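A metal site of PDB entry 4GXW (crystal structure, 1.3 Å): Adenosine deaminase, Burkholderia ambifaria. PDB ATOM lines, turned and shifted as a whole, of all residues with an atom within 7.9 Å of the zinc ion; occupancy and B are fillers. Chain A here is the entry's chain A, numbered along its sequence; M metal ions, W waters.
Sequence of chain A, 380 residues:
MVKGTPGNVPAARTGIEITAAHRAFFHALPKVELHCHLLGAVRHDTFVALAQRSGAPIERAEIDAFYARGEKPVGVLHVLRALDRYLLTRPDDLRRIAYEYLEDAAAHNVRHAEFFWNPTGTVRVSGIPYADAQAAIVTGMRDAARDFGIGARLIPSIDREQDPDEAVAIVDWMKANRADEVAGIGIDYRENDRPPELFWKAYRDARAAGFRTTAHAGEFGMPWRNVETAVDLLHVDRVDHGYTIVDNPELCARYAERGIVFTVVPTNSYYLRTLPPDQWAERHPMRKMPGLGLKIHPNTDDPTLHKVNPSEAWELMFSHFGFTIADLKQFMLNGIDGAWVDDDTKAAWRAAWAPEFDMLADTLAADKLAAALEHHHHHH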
ATOM      1  N   HIS A  35     -18.677  13.951  15.061  1.00  0.00           N
ATOM      2  CA  HIS A  35     -17.743  14.919  15.650  1.00  0.00           C
ATOM      3  C   HIS A  35     -16.370  14.285  15.790  1.00  0.00           C
ATOM      4  O   HIS A  35     -16.074  13.611  16.787  1.00  0.00           O
ATOM      5  CB  HIS A  35     -18.273  15.412  17.019  1.00  0.00           C
ATOM      6  CG  HIS A  35     -17.496  16.565  17.599  1.00  0.00           C
ATOM      7  ND1 HIS A  35     -18.069  17.479  18.446  1.00  0.00           N
ATOM      8  CD2 HIS A  35     -16.190  16.931  17.473  1.00  0.00           C
ATOM      9  CE1 HIS A  35     -17.158  18.382  18.805  1.00  0.00           C
ATOM     10  NE2 HIS A  35     -16.011  18.073  18.221  1.00  0.00           N
ATOM     11  N   CYS A  36     -15.553  14.494  14.772  1.00  0.00           N
ATOM     12  CA  CYS A  36     -14.204  13.948  14.750  1.00  0.00           C
ATOM     13  C   CYS A  36     -13.335  14.817  13.863  1.00  0.00           C
ATOM     14  O   CYS A  36     -13.678  15.074  12.704  1.00  0.00           O
ATOM     15  CB  CYS A  36     -14.205  12.517  14.202  1.00  0.00           C
ATOM     16  SG  CYS A  36     -12.582  11.753  14.283  1.00  0.00           S
ATOM     17  N   HIS A  37     -12.200  15.246  14.394  1.00  0.00           N
ATOM     18  CA  HIS A  37     -11.240  16.030  13.627  1.00  0.00           C
ATOM     19  C   HIS A  37     -10.237  15.096  12.977  1.00  0.00           C
ATOM     20  O   HIS A  37      -9.568  14.312  13.675  1.00  0.00           O
ATOM     21  CB  HIS A  37     -10.549  17.079  14.500  1.00  0.00           C
ATOM     22  CG  HIS A  37     -11.497  17.999  15.183  1.00  0.00           C
ATOM     23  ND1 HIS A  37     -11.860  19.234  14.657  1.00  0.00           N
ATOM     24  CD2 HIS A  37     -12.212  17.862  16.331  1.00  0.00           C
ATOM     25  CE1 HIS A  37     -12.735  19.808  15.463  1.00  0.00           C
ATOM     26  NE2 HIS A  37     -12.972  18.995  16.476  1.00  0.00           N
ATOM     27  N   LEU A  77      -4.787  21.092  20.548  1.00  0.00           N
ATOM     28  CA  LEU A  77      -4.804  21.981  19.386  1.00  0.00           C
ATOM     29  C   LEU A  77      -3.405  22.190  18.825  1.00  0.00           C
ATOM     30  O   LEU A  77      -3.222  22.313  17.605  1.00  0.00           O
ATOM     31  CB  LEU A  77      -5.488  23.304  19.723  1.00  0.00           C
ATOM     32  CG  LEU A  77      -6.943  23.176  20.170  1.00  0.00           C
ATOM     33  CD1 LEU A  77      -7.576  24.535  20.402  1.00  0.00           C
ATOM     34  CD2 LEU A  77      -7.757  22.373  19.160  1.00  0.00           C
ATOM     35  N   LEU A  80      -2.467  19.513  16.290  1.00  0.00           N
ATOM     36  CA  LEU A  80      -3.070  19.823  14.999  1.00  0.00           C
ATOM     37  C   LEU A  80      -2.249  20.884  14.286  1.00  0.00           C
ATOM     38  O   LEU A  80      -2.004  20.768  13.073  1.00  0.00           O
ATOM     39  CB  LEU A  80      -4.513  20.299  15.169  1.00  0.00           C
ATOM     40  CG  LEU A  80      -5.570  19.188  15.214  1.00  0.00           C
ATOM     41  CD1 LEU A  80      -5.420  18.298  16.436  1.00  0.00           C
ATOM     42  CD2 LEU A  80      -6.969  19.800  15.139  1.00  0.00           C
ATOM     43  N   PHE A 116     -14.199  16.609  10.442  1.00  0.00           N
ATOM     44  CA  PHE A 116     -13.767  17.996  10.274  1.00  0.00           C
ATOM     45  C   PHE A 116     -12.329  18.098   9.736  1.00  0.00           C
ATOM     46  O   PHE A 116     -11.436  17.361  10.161  1.00  0.00           O
ATOM     47  CB  PHE A 116     -13.799  18.722  11.620  1.00  0.00           C
ATOM     48  CG  PHE A 116     -15.163  18.780  12.276  1.00  0.00           C
ATOM     49  CD1 PHE A 116     -16.287  19.189  11.577  1.00  0.00           C
ATOM     50  CD2 PHE A 116     -15.310  18.417  13.612  1.00  0.00           C
ATOM     51  CE1 PHE A 116     -17.531  19.236  12.207  1.00  0.00           C
ATOM     52  CE2 PHE A 116     -16.555  18.486  14.236  1.00  0.00           C
ATOM     53  CZ  PHE A 116     -17.667  18.892  13.519  1.00  0.00           C
ATOM     54  N   ILE A 187     -17.110  25.145  12.579  1.00  0.00           N
ATOM     55  CA  ILE A 187     -16.166  26.131  13.110  1.00  0.00           C
ATOM     56  C   ILE A 187     -15.556  25.566  14.386  1.00  0.00           C
ATOM     57  O   ILE A 187     -16.273  25.032  15.242  1.00  0.00           O
ATOM     58  CB  ILE A 187     -16.827  27.519  13.354  1.00  0.00           C
ATOM     59  CG1 ILE A 187     -15.774  28.541  13.767  1.00  0.00           C
ATOM     60  CG2 ILE A 187     -17.927  27.459  14.414  1.00  0.00           C
ATOM     61  CD1 ILE A 187     -16.270  29.982  13.676  1.00  0.00           C
ATOM     62  N   ASP A 188     -14.235  25.658  14.510  1.00  0.00           N
ATOM     63  CA  ASP A 188     -13.542  25.115  15.673  1.00  0.00           C
ATOM     64  C   ASP A 188     -12.268  25.906  15.983  1.00  0.00           C
ATOM     65  O   ASP A 188     -12.115  27.040  15.524  1.00  0.00           O
ATOM     66  CB  ASP A 188     -13.298  23.606  15.522  1.00  0.00           C
ATOM     67  CG  ASP A 188     -12.569  23.248  14.228  1.00  0.00           C
ATOM     68  OD1 ASP A 188     -11.568  23.897  13.889  1.00  0.00           O
ATOM     69  OD2 ASP A 188     -13.013  22.290  13.556  1.00  0.00           O
ATOM     70  N   TYR A 189     -11.358  25.283  16.736  1.00  0.00           N
ATOM     71  CA  TYR A 189     -10.228  25.931  17.404  1.00  0.00           C
ATOM     72  C   TYR A 189     -10.685  26.745  18.628  1.00  0.00           C
ATOM     73  O   TYR A 189     -11.829  26.578  19.072  1.00  0.00           O
ATOM     74  CB  TYR A 189      -9.292  26.672  16.435  1.00  0.00           C
ATOM     75  CG  TYR A 189      -8.308  25.754  15.716  1.00  0.00           C
ATOM     76  CD1 TYR A 189      -7.211  25.242  16.388  1.00  0.00           C
ATOM     77  CD2 TYR A 189      -8.475  25.414  14.378  1.00  0.00           C
ATOM     78  CE1 TYR A 189      -6.303  24.413  15.763  1.00  0.00           C
ATOM     79  CE2 TYR A 189      -7.541  24.578  13.735  1.00  0.00           C
ATOM     80  CZ  TYR A 189      -6.474  24.087  14.442  1.00  0.00           C
ATOM     81  OH  TYR A 189      -5.526  23.269  13.845  1.00  0.00           O
ATOM     82  N   HIS A 216     -18.977  24.525  16.732  1.00  0.00           N
ATOM     83  CA  HIS A 216     -18.549  24.371  18.125  1.00  0.00           C
ATOM     84  C   HIS A 216     -19.057  25.596  18.897  1.00  0.00           C
ATOM     85  O   HIS A 216     -18.804  26.744  18.505  1.00  0.00           O
ATOM     86  CB  HIS A 216     -17.015  24.302  18.238  1.00  0.00           C
ATOM     87  CG  HIS A 216     -16.403  22.988  17.839  1.00  0.00           C
ATOM     88  ND1 HIS A 216     -16.632  22.375  16.626  1.00  0.00           N
ATOM     89  CD2 HIS A 216     -15.530  22.180  18.503  1.00  0.00           C
ATOM     90  CE1 HIS A 216     -15.950  21.242  16.558  1.00  0.00           C
ATOM     91  NE2 HIS A 216     -15.271  21.100  17.690  1.00  0.00           N
ATOM     92  N   GLU A 219     -18.134  25.464  24.515  1.00  0.00           N
ATOM     93  CA  GLU A 219     -16.972  24.743  25.014  1.00  0.00           C
ATOM     94  C   GLU A 219     -16.115  25.697  25.849  1.00  0.00           C
ATOM     95  O   GLU A 219     -16.296  26.916  25.786  1.00  0.00           O
ATOM     96  CB  GLU A 219     -16.147  24.184  23.840  1.00  0.00           C
ATOM     97  CG  GLU A 219     -15.127  23.122  24.230  1.00  0.00           C
ATOM     98  CD  GLU A 219     -14.294  22.595  23.068  1.00  0.00           C
ATOM     99  OE1 GLU A 219     -14.464  23.039  21.908  1.00  0.00           O
ATOM    100  OE2 GLU A 219     -13.423  21.735  23.322  1.00  0.00           O
ATOM    101  N   ASP A 240     -22.120  21.469  17.961  1.00  0.00           N
ATOM    102  CA  ASP A 240     -21.012  20.725  18.548  1.00  0.00           C
ATOM    103  C   ASP A 240     -20.697  21.201  19.962  1.00  0.00           C
ATOM    104  O   ASP A 240     -20.432  22.389  20.187  1.00  0.00           O
ATOM    105  CB  ASP A 240     -19.792  20.759  17.629  1.00  0.00           C
ATOM    106  CG  ASP A 240     -20.100  20.219  16.251  1.00  0.00           C
ATOM    107  OD1 ASP A 240     -20.554  19.053  16.146  1.00  0.00           O
ATOM    108  OD2 ASP A 240     -19.937  20.997  15.269  1.00  0.00           O
ATOM    109  N   HIS A 241     -20.762  20.245  20.890  1.00  0.00           N
ATOM    110  CA  HIS A 241     -20.607  20.442  22.339  1.00  0.00           C
ATOM    111  C   HIS A 241     -21.878  21.032  22.936  1.00  0.00           C
ATOM    112  O   HIS A 241     -22.799  20.295  23.304  1.00  0.00           O
ATOM    113  CB  HIS A 241     -19.360  21.262  22.713  1.00  0.00           C
ATOM    114  CG  HIS A 241     -18.055  20.645  22.295  1.00  0.00           C
ATOM    115  ND1 HIS A 241     -17.668  19.373  22.693  1.00  0.00           N
ATOM    116  CD2 HIS A 241     -17.042  21.128  21.534  1.00  0.00           C
ATOM    117  CE1 HIS A 241     -16.469  19.115  22.193  1.00  0.00           C
ATOM    118  NE2 HIS A 241     -16.065  20.172  21.492  1.00  0.00           N
ATOM    119  N   THR A 263     -23.700  17.267  19.403  1.00  0.00           N
ATOM    120  CA  THR A 263     -22.662  16.254  19.440  1.00  0.00           C
ATOM    121  C   THR A 263     -21.881  16.484  20.727  1.00  0.00           C
ATOM    122  O   THR A 263     -21.547  17.617  21.072  1.00  0.00           O
ATOM    123  CB  THR A 263     -21.747  16.299  18.184  1.00  0.00           C
ATOM    124  OG1 THR A 263     -20.940  17.481  18.203  1.00  0.00           O
ATOM    125  CG2 THR A 263     -22.574  16.255  16.908  1.00  0.00           C
ATOM    126  N   VAL A 265     -18.802  14.963  23.680  1.00  0.00           N
ATOM    127  CA  VAL A 265     -17.507  14.292  23.730  1.00  0.00           C
ATOM    128  C   VAL A 265     -17.185  14.007  25.184  1.00  0.00           C
ATOM    129  O   VAL A 265     -16.791  14.908  25.934  1.00  0.00           O
ATOM    130  CB  VAL A 265     -16.418  15.192  23.091  1.00  0.00           C
ATOM    131  CG1 VAL A 265     -15.052  14.511  23.150  1.00  0.00           C
ATOM    132  CG2 VAL A 265     -16.784  15.560  21.648  1.00  0.00           C
ATOM    133  N   ASN A 268     -13.913  15.310  26.583  1.00  0.00           N
ATOM    134  CA  ASN A 268     -13.626  16.731  26.430  1.00  0.00           C
ATOM    135  C   ASN A 268     -12.511  17.184  27.360  1.00  0.00           C
ATOM    136  O   ASN A 268     -12.605  17.013  28.577  1.00  0.00           O
ATOM    137  CB  ASN A 268     -14.890  17.550  26.673  1.00  0.00           C
ATOM    138  CG  ASN A 268     -14.648  19.046  26.555  1.00  0.00           C
ATOM    139  OD1 ASN A 268     -14.612  19.753  27.559  1.00  0.00           O
ATOM    140  ND2 ASN A 268     -14.488  19.529  25.317  1.00  0.00           N
ATOM    141  N   THR A 300     -15.870  10.794  19.496  1.00  0.00           N
ATOM    142  CA  THR A 300     -14.482  10.743  19.960  1.00  0.00           C
ATOM    143  C   THR A 300     -13.716  12.061  19.892  1.00  0.00           C
ATOM    144  O   THR A 300     -12.781  12.260  20.679  1.00  0.00           O
ATOM    145  CB  THR A 300     -13.656   9.642  19.218  1.00  0.00           C
ATOM    146  OG1 THR A 300     -13.602   9.935  17.810  1.00  0.00           O
ATOM    147  CG2 THR A 300     -14.249   8.248  19.442  1.00  0.00           C
ATOM    148  N   ASP A 301     -14.078  12.951  18.960  1.00  0.00           N
ATOM    149  CA  ASP A 301     -13.430  14.273  18.757  1.00  0.00           C
ATOM    150  C   ASP A 301     -12.008  14.150  18.187  1.00  0.00           C
ATOM    151  O   ASP A 301     -11.769  14.508  17.027  1.00  0.00           O
ATOM    152  CB  ASP A 301     -13.462  15.115  20.039  1.00  0.00           C
ATOM    153  CG  ASP A 301     -13.432  16.649  19.818  1.00  0.00           C
ATOM    154  OD1 ASP A 301     -13.486  17.198  18.682  1.00  0.00           O
ATOM    155  OD2 ASP A 301     -13.390  17.350  20.850  1.00  0.00           O
ATOM    156  N   ASP A 302     -11.085  13.656  18.996  1.00  0.00           N
ATOM    157  CA  ASP A 302      -9.693  13.459  18.572  1.00  0.00           C
ATOM    158  C   ASP A 302      -9.270  12.065  19.039  1.00  0.00           C
ATOM    159  O   ASP A 302      -8.545  11.942  20.042  1.00  0.00           O
ATOM    160  CB  ASP A 302      -8.763  14.521  19.184  1.00  0.00           C
ATOM    161  CG  ASP A 302      -9.207  15.932  18.867  1.00  0.00           C
ATOM    162  OD1 ASP A 302      -8.993  16.386  17.725  1.00  0.00           O
ATOM    163  OD2 ASP A 302      -9.769  16.599  19.761  1.00  0.00           O
ATOM    164  N   HIS A 306      -6.868  11.685  22.174  1.00  0.00           N
ATOM    165  CA  HIS A 306      -7.618  11.487  23.416  1.00  0.00           C
ATOM    166  C   HIS A 306      -7.531  10.037  23.905  1.00  0.00           C
ATOM    167  O   HIS A 306      -7.991   9.735  25.001  1.00  0.00           O
ATOM    168  CB  HIS A 306      -9.096  11.836  23.235  1.00  0.00           C
ATOM    169  CG  HIS A 306      -9.386  13.303  23.197  1.00  0.00           C
ATOM    170  ND1 HIS A 306     -10.653  13.806  23.390  1.00  0.00           N
ATOM    171  CD2 HIS A 306      -8.586  14.374  22.980  1.00  0.00           C
ATOM    172  CE1 HIS A 306     -10.625  15.126  23.292  1.00  0.00           C
ATOM    173  NE2 HIS A 306      -9.374  15.492  23.045  1.00  0.00           N
HETATM  174 ZN    ZN M   1     -14.161  19.197  18.177  1.00  0.00          ZN
HETATM  175  O   HOH W   1     -13.770  19.812  20.003  1.00  0.00           O
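A ring nitrogen (ND1) of His 35 lies within hydrogen-bond range of the side-chain hydroxyl (OG1) of Thr 263 (2.9 Å). A ring nitrogen (ND1) of His 37 sits close to the side-chain carboxylate (OD2) of Asp 188 (3.4 Å). The backbone carbonyl oxygen (O) of Ile 187 sits at hydrogen-bond distance from a ring nitrogen (ND1) of His 216 (3.0 Å). The backbone NH of His 241 sits at hydrogen-bond distance from the backbone carbonyl oxygen of Thr 263, 2.7 Å away. NE2 of His 241 lies close to OE1 of Glu 219 (3.3 Å).
His 241 touches the zinc ion. Along chain A the residues within 4 Å of the zinc ion span positions 35 to 301. The nearest printed residue that does not touch the zinc ion is Phe 116 (4.7 Å).
The zinc ion is bound by water W1 (2.0 Å), NE2 of His 37 (2.1 Å), NE2 of His 35 (2.2 Å), OD1 of Asp 301 (2.2 Å) and NE2 of His 216 (2.3 Å). The zinc ion has five donor atoms within binding distance.
Water W1 bridges the side-chain carboxylate (OD2) of Asp 301 (2.6 Å) and a ring nitrogen (NE2) of His 241 (2.8 Å).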
